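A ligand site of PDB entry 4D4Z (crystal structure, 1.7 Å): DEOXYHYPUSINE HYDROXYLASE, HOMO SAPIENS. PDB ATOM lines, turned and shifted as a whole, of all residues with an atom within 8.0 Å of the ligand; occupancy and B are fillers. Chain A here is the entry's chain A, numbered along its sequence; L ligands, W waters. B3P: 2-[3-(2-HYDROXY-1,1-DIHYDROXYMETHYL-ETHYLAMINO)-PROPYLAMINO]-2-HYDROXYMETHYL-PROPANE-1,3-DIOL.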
ATOM      1  N   ILE A  48     -29.555  -3.446   8.722  1.00  0.00           N
ATOM      2  CA  ILE A  48     -28.465  -4.186   9.392  1.00  0.00           C
ATOM      3  C   ILE A  48     -27.264  -4.112   8.457  1.00  0.00           C
ATOM      4  O   ILE A  48     -26.114  -3.822   8.843  1.00  0.00           O
ATOM      5  CB  ILE A  48     -28.877  -5.624   9.718  1.00  0.00           C
ATOM      6  CG1 ILE A  48     -29.962  -5.575  10.822  1.00  0.00           C
ATOM      7  CG2 ILE A  48     -27.666  -6.475  10.160  1.00  0.00           C
ATOM      8  CD1 ILE A  48     -30.668  -6.904  11.086  1.00  0.00           C
ATOM      9  N   SER A  49     -27.521  -4.419   7.179  1.00  0.00           N
ATOM     10  CA  SER A  49     -26.405  -4.479   6.180  1.00  0.00           C
ATOM     11  C   SER A  49     -25.694  -3.145   6.007  1.00  0.00           C
ATOM     12  O   SER A  49     -24.482  -3.123   5.743  1.00  0.00           O
ATOM     13  CB  SER A  49     -26.905  -4.954   4.848  1.00  0.00           C
ATOM     14  OG  SER A  49     -27.418  -6.244   4.859  1.00  0.00           O
ATOM     15  N   GLN A  50     -26.408  -2.039   6.173  1.00  0.00           N
ATOM     16  CA  GLN A  50     -25.869  -0.696   6.014  1.00  0.00           C
ATOM     17  C   GLN A  50     -24.783  -0.391   7.064  1.00  0.00           C
ATOM     18  O   GLN A  50     -23.875   0.387   6.763  1.00  0.00           O
ATOM     19  CB  GLN A  50     -26.996   0.369   6.018  1.00  0.00           C
ATOM     20  CG  GLN A  50     -26.506   1.715   5.684  1.00  0.00           C
ATOM     21  CD  GLN A  50     -27.619   2.735   5.708  1.00  0.00           C
ATOM     22  OE1 GLN A  50     -28.689   2.501   5.141  1.00  0.00           O
ATOM     23  NE2 GLN A  50     -27.357   3.854   6.287  1.00  0.00           N
ATOM     24  N   ALA A  51     -24.819  -1.027   8.254  1.00  0.00           N
ATOM     25  CA  ALA A  51     -23.898  -0.702   9.319  1.00  0.00           C
ATOM     26  C   ALA A  51     -22.528  -1.434   9.206  1.00  0.00           C
ATOM     27  O   ALA A  51     -21.692  -1.257  10.070  1.00  0.00           O
ATOM     28  CB  ALA A  51     -24.587  -1.039  10.679  1.00  0.00           C
ATOM     29  N   PHE A  52     -22.312  -2.250   8.148  1.00  0.00           N
ATOM     30  CA  PHE A  52     -21.069  -3.022   7.981  1.00  0.00           C
ATOM     31  C   PHE A  52     -19.793  -2.224   7.732  1.00  0.00           C
ATOM     32  O   PHE A  52     -18.718  -2.823   7.596  1.00  0.00           O
ATOM     33  CB  PHE A  52     -21.192  -4.093   6.943  1.00  0.00           C
ATOM     34  CG  PHE A  52     -21.679  -5.403   7.436  1.00  0.00           C
ATOM     35  CD1 PHE A  52     -20.924  -6.150   8.379  1.00  0.00           C
ATOM     36  CD2 PHE A  52     -22.851  -5.943   6.977  1.00  0.00           C
ATOM     37  CE1 PHE A  52     -21.432  -7.359   8.833  1.00  0.00           C
ATOM     38  CE2 PHE A  52     -23.327  -7.155   7.422  1.00  0.00           C
ATOM     39  CZ  PHE A  52     -22.607  -7.871   8.365  1.00  0.00           C
ATOM     40  N   ASP A  53     -19.931  -0.935   7.606  1.00  0.00           N
ATOM     41  CA  ASP A  53     -18.679  -0.164   7.581  1.00  0.00           C
ATOM     42  C   ASP A  53     -18.467   0.754   8.757  1.00  0.00           C
ATOM     43  O   ASP A  53     -17.604   1.629   8.783  1.00  0.00           O
ATOM     44  CB  ASP A  53     -18.519   0.511   6.263  1.00  0.00           C
ATOM     45  CG  ASP A  53     -18.484  -0.509   5.106  1.00  0.00           C
ATOM     46  OD1 ASP A  53     -17.678  -1.531   5.051  1.00  0.00           O
ATOM     47  OD2 ASP A  53     -19.372  -0.266   4.268  1.00  0.00           O
ATOM     48  N   ASP A  54     -19.102   0.370   9.848  1.00  0.00           N
ATOM     49  CA  ASP A  54     -18.811   1.037  11.091  1.00  0.00           C
ATOM     50  C   ASP A  54     -17.384   0.778  11.573  1.00  0.00           C
ATOM     51  O   ASP A  54     -16.768  -0.252  11.236  1.00  0.00           O
ATOM     52  CB  ASP A  54     -19.813   0.547  12.138  1.00  0.00           C
ATOM     53  CG  ASP A  54     -19.850   1.432  13.307  1.00  0.00           C
ATOM     54  OD1 ASP A  54     -20.491   2.480  13.187  1.00  0.00           O
ATOM     55  OD2 ASP A  54     -19.264   1.121  14.390  1.00  0.00           O
ATOM     56  N   LYS A  60     -19.912  -4.661  14.081  1.00  0.00           N
ATOM     57  CA  LYS A  60     -19.963  -5.279  12.794  1.00  0.00           C
ATOM     58  C   LYS A  60     -20.164  -6.799  12.858  1.00  0.00           C
ATOM     59  O   LYS A  60     -20.946  -7.376  12.133  1.00  0.00           O
ATOM     60  CB  LYS A  60     -18.698  -4.965  11.938  1.00  0.00           C
ATOM     61  CG  LYS A  60     -18.699  -3.527  11.458  1.00  0.00           C
ATOM     62  CD  LYS A  60     -17.545  -3.319  10.505  1.00  0.00           C
ATOM     63  CE  LYS A  60     -16.245  -3.379  11.199  1.00  0.00           C
ATOM     64  NZ  LYS A  60     -15.118  -3.179  10.234  1.00  0.00           N
ATOM     65  N   LEU A  63     -23.698  -7.667  13.667  1.00  0.00           N
ATOM     66  CA  LEU A  63     -24.552  -7.587  12.476  1.00  0.00           C
ATOM     67  C   LEU A  63     -24.607  -8.914  11.771  1.00  0.00           C
ATOM     68  O   LEU A  63     -25.656  -9.450  11.428  1.00  0.00           O
ATOM     69  CB  LEU A  63     -24.090  -6.508  11.477  1.00  0.00           C
ATOM     70  CG  LEU A  63     -23.869  -5.167  12.026  1.00  0.00           C
ATOM     71  CD1 LEU A  63     -23.185  -4.355  10.886  1.00  0.00           C
ATOM     72  CD2 LEU A  63     -25.123  -4.485  12.467  1.00  0.00           C
ATOM     73  N   PRO A  77     -26.002 -12.298  -0.039  1.00  0.00           N
ATOM     74  CA  PRO A  77     -25.042 -11.462  -0.751  1.00  0.00           C
ATOM     75  C   PRO A  77     -24.153 -10.584   0.096  1.00  0.00           C
ATOM     76  O   PRO A  77     -22.926 -10.526  -0.107  1.00  0.00           O
ATOM     77  CB  PRO A  77     -25.935 -10.604  -1.650  1.00  0.00           C
ATOM     78  CG  PRO A  77     -27.108 -11.496  -1.922  1.00  0.00           C
ATOM     79  CD  PRO A  77     -27.367 -12.200  -0.592  1.00  0.00           C
ATOM     80  N   MET A  78     -24.723  -9.914   1.080  1.00  0.00           N
ATOM     81  CA  MET A  78     -23.937  -9.075   1.975  1.00  0.00           C
ATOM     82  C   MET A  78     -22.946  -9.890   2.818  1.00  0.00           C
ATOM     83  O   MET A  78     -21.789  -9.471   3.003  1.00  0.00           O
ATOM     84  CB  MET A  78     -24.805  -8.249   2.899  1.00  0.00           C
ATOM     85  CG  MET A  78     -24.016  -7.305   3.833  1.00  0.00           C
ATOM     86  SD  MET A  78     -22.738  -6.209   2.990  1.00  0.00           S
ATOM     87  CE  MET A  78     -23.871  -4.955   2.466  1.00  0.00           C
ATOM     88  N   LEU A  79     -23.399 -11.021   3.328  1.00  0.00           N
ATOM     89  CA  LEU A  79     -22.540 -11.882   4.105  1.00  0.00           C
ATOM     90  C   LEU A  79     -21.315 -12.388   3.275  1.00  0.00           C
ATOM     91  O   LEU A  79     -20.188 -12.421   3.773  1.00  0.00           O
ATOM     92  CB  LEU A  79     -23.294 -13.038   4.724  1.00  0.00           C
ATOM     93  CG  LEU A  79     -24.277 -12.596   5.790  1.00  0.00           C
ATOM     94  CD1 LEU A  79     -25.155 -13.824   6.090  1.00  0.00           C
ATOM     95  CD2 LEU A  79     -23.549 -12.121   7.061  1.00  0.00           C
ATOM     96  N   VAL A  80     -21.576 -12.703   2.009  1.00  0.00           N
ATOM     97  CA  VAL A  80     -20.498 -13.074   1.099  1.00  0.00           C
ATOM     98  C   VAL A  80     -19.509 -11.921   0.947  1.00  0.00           C
ATOM     99  O   VAL A  80     -18.261 -12.110   1.036  1.00  0.00           O
ATOM    100  CB  VAL A  80     -21.075 -13.593  -0.231  1.00  0.00           C
ATOM    101  CG1 VAL A  80     -19.948 -13.637  -1.295  1.00  0.00           C
ATOM    102  CG2 VAL A  80     -21.797 -14.944  -0.071  1.00  0.00           C
ATOM    103  N   ASP A  81     -19.977 -10.695   0.670  1.00  0.00           N
ATOM    104  CA  ASP A  81     -19.115  -9.522   0.562  1.00  0.00           C
ATOM    105  C   ASP A  81     -18.281  -9.262   1.784  1.00  0.00           C
ATOM    106  O   ASP A  81     -17.102  -8.926   1.676  1.00  0.00           O
ATOM    107  CB  ASP A  81     -19.895  -8.297   0.192  1.00  0.00           C
ATOM    108  CG  ASP A  81     -20.391  -8.324  -1.292  1.00  0.00           C
ATOM    109  OD1 ASP A  81     -19.987  -9.198  -2.074  1.00  0.00           O
ATOM    110  OD2 ASP A  81     -21.124  -7.378  -1.613  1.00  0.00           O
ATOM    111  N   VAL A  82     -18.852  -9.442   2.975  1.00  0.00           N
ATOM    112  CA  VAL A  82     -18.120  -9.319   4.195  1.00  0.00           C
ATOM    113  C   VAL A  82     -17.073 -10.404   4.352  1.00  0.00           C
ATOM    114  O   VAL A  82     -15.912 -10.057   4.681  1.00  0.00           O
ATOM    115  CB  VAL A  82     -19.037  -9.276   5.379  1.00  0.00           C
ATOM    116  CG1 VAL A  82     -18.257  -9.240   6.678  1.00  0.00           C
ATOM    117  CG2 VAL A  82     -19.898  -8.023   5.326  1.00  0.00           C
ATOM    118  N   LEU A  83     -17.399 -11.634   4.113  1.00  0.00           N
ATOM    119  CA  LEU A  83     -16.430 -12.749   4.229  1.00  0.00           C
ATOM    120  C   LEU A  83     -15.238 -12.491   3.275  1.00  0.00           C
ATOM    121  O   LEU A  83     -14.073 -12.757   3.642  1.00  0.00           O
ATOM    122  CB  LEU A  83     -17.097 -14.027   3.852  1.00  0.00           C
ATOM    123  CG  LEU A  83     -16.291 -15.261   3.703  1.00  0.00           C
ATOM    124  CD1 LEU A  83     -15.511 -15.536   4.976  1.00  0.00           C
ATOM    125  CD2 LEU A  83     -17.076 -16.464   3.235  1.00  0.00           C
ATOM    126  N   GLN A  84     -15.544 -12.006   2.082  1.00  0.00           N
ATOM    127  CA  GLN A  84     -14.435 -11.816   1.071  1.00  0.00           C
ATOM    128  C   GLN A  84     -13.655 -10.573   1.288  1.00  0.00           C
ATOM    129  O   GLN A  84     -12.596 -10.435   0.598  1.00  0.00           O
ATOM    130  CB  GLN A  84     -15.027 -11.780  -0.318  1.00  0.00           C
ATOM    131  CG  GLN A  84     -15.725 -13.055  -0.685  1.00  0.00           C
ATOM    132  CD  GLN A  84     -15.842 -13.257  -2.200  1.00  0.00           C
ATOM    133  OE1 GLN A  84     -16.641 -12.578  -2.874  1.00  0.00           O
ATOM    134  NE2 GLN A  84     -14.921 -14.036  -2.755  1.00  0.00           N
ATOM    135  N   ASP A  85     -14.087  -9.650   2.101  1.00  0.00           N
ATOM    136  CA  ASP A  85     -13.423  -8.354   2.265  1.00  0.00           C
ATOM    137  C   ASP A  85     -12.247  -8.538   3.214  1.00  0.00           C
ATOM    138  O   ASP A  85     -12.398  -8.564   4.452  1.00  0.00           O
ATOM    139  CB  ASP A  85     -14.363  -7.325   2.805  1.00  0.00           C
ATOM    140  CG  ASP A  85     -13.726  -5.947   3.004  1.00  0.00           C
ATOM    141  OD1 ASP A  85     -12.530  -5.727   2.617  1.00  0.00           O
ATOM    142  OD2 ASP A  85     -14.450  -5.053   3.474  1.00  0.00           O
ATOM    143  N   THR A  86     -11.023  -8.586   2.673  1.00  0.00           N
ATOM    144  CA  THR A  86      -9.891  -8.794   3.534  1.00  0.00           C
ATOM    145  C   THR A  86      -9.530  -7.624   4.464  1.00  0.00           C
ATOM    146  O   THR A  86      -8.677  -7.794   5.310  1.00  0.00           O
ATOM    147  CB  THR A  86      -8.647  -9.228   2.703  1.00  0.00           C
ATOM    148  OG1 THR A  86      -8.300  -8.134   1.918  1.00  0.00           O
ATOM    149  CG2 THR A  86      -8.930 -10.447   1.852  1.00  0.00           C
ATOM    150  N   ARG A  87     -10.082  -6.427   4.282  1.00  0.00           N
ATOM    151  CA  ARG A  87      -9.959  -5.337   5.187  1.00  0.00           C
ATOM    152  C   ARG A  87     -10.854  -5.464   6.427  1.00  0.00           C
ATOM    153  O   ARG A  87     -10.627  -4.761   7.417  1.00  0.00           O
ATOM    154  CB  ARG A  87     -10.320  -4.048   4.518  1.00  0.00           C
ATOM    155  CG  ARG A  87      -9.373  -3.684   3.378  1.00  0.00           C
ATOM    156  CD  ARG A  87      -9.270  -2.175   3.296  1.00  0.00           C
ATOM    157  NE  ARG A  87      -8.345  -1.851   2.201  1.00  0.00           N
ATOM    158  CZ  ARG A  87      -8.212  -0.641   1.698  1.00  0.00           C
ATOM    159  NH1 ARG A  87      -8.899   0.378   2.220  1.00  0.00           N
ATOM    160  NH2 ARG A  87      -7.379  -0.474   0.677  1.00  0.00           N
ATOM    161  N   GLN A  88     -11.858  -6.339   6.376  1.00  0.00           N
ATOM    162  CA  GLN A  88     -12.610  -6.615   7.601  1.00  0.00           C
ATOM    163  C   GLN A  88     -11.792  -7.391   8.605  1.00  0.00           C
ATOM    164  O   GLN A  88     -10.948  -8.214   8.274  1.00  0.00           O
ATOM    165  CB  GLN A  88     -13.934  -7.372   7.289  1.00  0.00           C
ATOM    166  CG  GLN A  88     -14.947  -6.589   6.498  1.00  0.00           C
ATOM    167  CD  GLN A  88     -15.804  -5.644   7.318  1.00  0.00           C
ATOM    168  OE1 GLN A  88     -16.814  -5.062   6.814  1.00  0.00           O
ATOM    169  NE2 GLN A  88     -15.427  -5.450   8.511  1.00  0.00           N
ATOM    170  N   VAL A  92     -14.905 -10.373  12.235  1.00  0.00           N
ATOM    171  CA  VAL A  92     -16.083  -9.947  11.450  1.00  0.00           C
ATOM    172  C   VAL A  92     -16.230 -10.921  10.241  1.00  0.00           C
ATOM    173  O   VAL A  92     -17.333 -11.409   9.946  1.00  0.00           O
ATOM    174  CB  VAL A  92     -15.979  -8.531  10.927  1.00  0.00           C
ATOM    175  CG1 VAL A  92     -17.113  -8.199  10.012  1.00  0.00           C
ATOM    176  CG2 VAL A  92     -15.885  -7.536  12.091  1.00  0.00           C
ATOM    177  N   ARG A  93     -15.109 -11.240   9.590  1.00  0.00           N
ATOM    178  CA  ARG A  93     -15.142 -12.240   8.527  1.00  0.00           C
ATOM    179  C   ARG A  93     -15.562 -13.659   8.998  1.00  0.00           C
ATOM    180  O   ARG A  93     -16.380 -14.371   8.359  1.00  0.00           O
ATOM    181  CB  ARG A  93     -13.779 -12.280   7.817  1.00  0.00           C
ATOM    182  CG  ARG A  93     -13.330 -10.979   7.214  1.00  0.00           C
ATOM    183  CD  ARG A  93     -11.953 -11.020   6.508  1.00  0.00           C
ATOM    184  NE  ARG A  93     -11.991 -11.910   5.374  1.00  0.00           N
ATOM    185  CZ  ARG A  93     -11.111 -12.806   5.034  1.00  0.00           C
ATOM    186  NH1 ARG A  93      -9.896 -12.780   5.567  1.00  0.00           N
ATOM    187  NH2 ARG A  93     -11.365 -13.601   4.039  1.00  0.00           N
HETATM  188  C1  B3P L   1     -16.135  -1.568   1.844  1.00  0.00           C
HETATM  189  C2  B3P L   1     -16.942  -0.677   0.905  1.00  0.00           C
HETATM  190  C3  B3P L   1     -16.716  -2.982   1.759  1.00  0.00           C
HETATM  191  N1  B3P L   1     -17.909  -3.028   2.586  1.00  0.00           N
HETATM  192  C4  B3P L   1     -18.730  -4.206   2.652  1.00  0.00           C
HETATM  193  C5  B3P L   1     -19.700  -4.360   1.523  1.00  0.00           C
HETATM  194  C6  B3P L   1     -17.958  -5.521   2.836  1.00  0.00           C
HETATM  195  C7  B3P L   1     -19.695  -3.911   3.813  1.00  0.00           C
HETATM  196  N2  B3P L   1     -18.265  -0.354   1.432  1.00  0.00           N
HETATM  197  C8  B3P L   1     -19.246   0.296   0.576  1.00  0.00           C
HETATM  198  C9  B3P L   1     -19.456  -0.356  -0.779  1.00  0.00           C
HETATM  199  C10 B3P L   1     -20.539   0.295   1.349  1.00  0.00           C
HETATM  200  C11 B3P L   1     -18.794   1.702   0.234  1.00  0.00           C
HETATM  201  O1  B3P L   1     -19.846  -1.714  -0.688  1.00  0.00           O
HETATM  202  O2  B3P L   1     -21.489   1.004   0.556  1.00  0.00           O
HETATM  203  O3  B3P L   1     -18.122   2.350   1.278  1.00  0.00           O
HETATM  204  O4  B3P L   1     -18.997  -4.696   0.346  1.00  0.00           O
HETATM  205  O5  B3P L   1     -17.060  -5.375   3.905  1.00  0.00           O
HETATM  206  O6  B3P L   1     -20.442  -2.715   3.538  1.00  0.00           O
HETATM  207  O   HOH W   1     -22.745  -1.784   4.063  1.00  0.00           O
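A nitrogen (N1) of the ligand is in salt-bridge range of the side-chain carboxylate of Asp 53, at 2.9 Å.
The side-chain carboxylate (OD2) of Asp 85 is in hydrogen-bond range of an oxygen (O5) of the ligand (2.7 Å).
The side-chain amide oxygen (OE1) of Gln 88 sits at hydrogen-bond distance from an oxygen (O5) of the ligand (2.9 Å).
NE of Arg 93 sits close to O of Asp 85, 3.5 Å away.
OD1 of Asp 85 is in hydrogen-bond range of N of Arg 87 (3.0 Å).
The side-chain amide oxygen (OE1) of Gln 88 sits close to the backbone carbonyl oxygen (O) of Phe 52 (3.0 Å).
The side-chain amide nitrogen (NE2) of Gln 88 lies close to the side-chain amino group (NZ) of Lys 60.
Merely in contact with the ligand: Phe 52, Asp 81 and Met 78.
Hydrophobic or aromatic side chains that line the ligand: Phe 52 and Met 78.
Within 4 Å of the ligand: Phe 52, Asp 53, Met 78, Asp 81, Asp 85 and Gln 88.
Water W1 lies within hydrogen-bond range of an oxygen (O6) of the ligand (2.5 Å) and the backbone carbonyl oxygen (O) of Ser 49 (2.8 Å).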
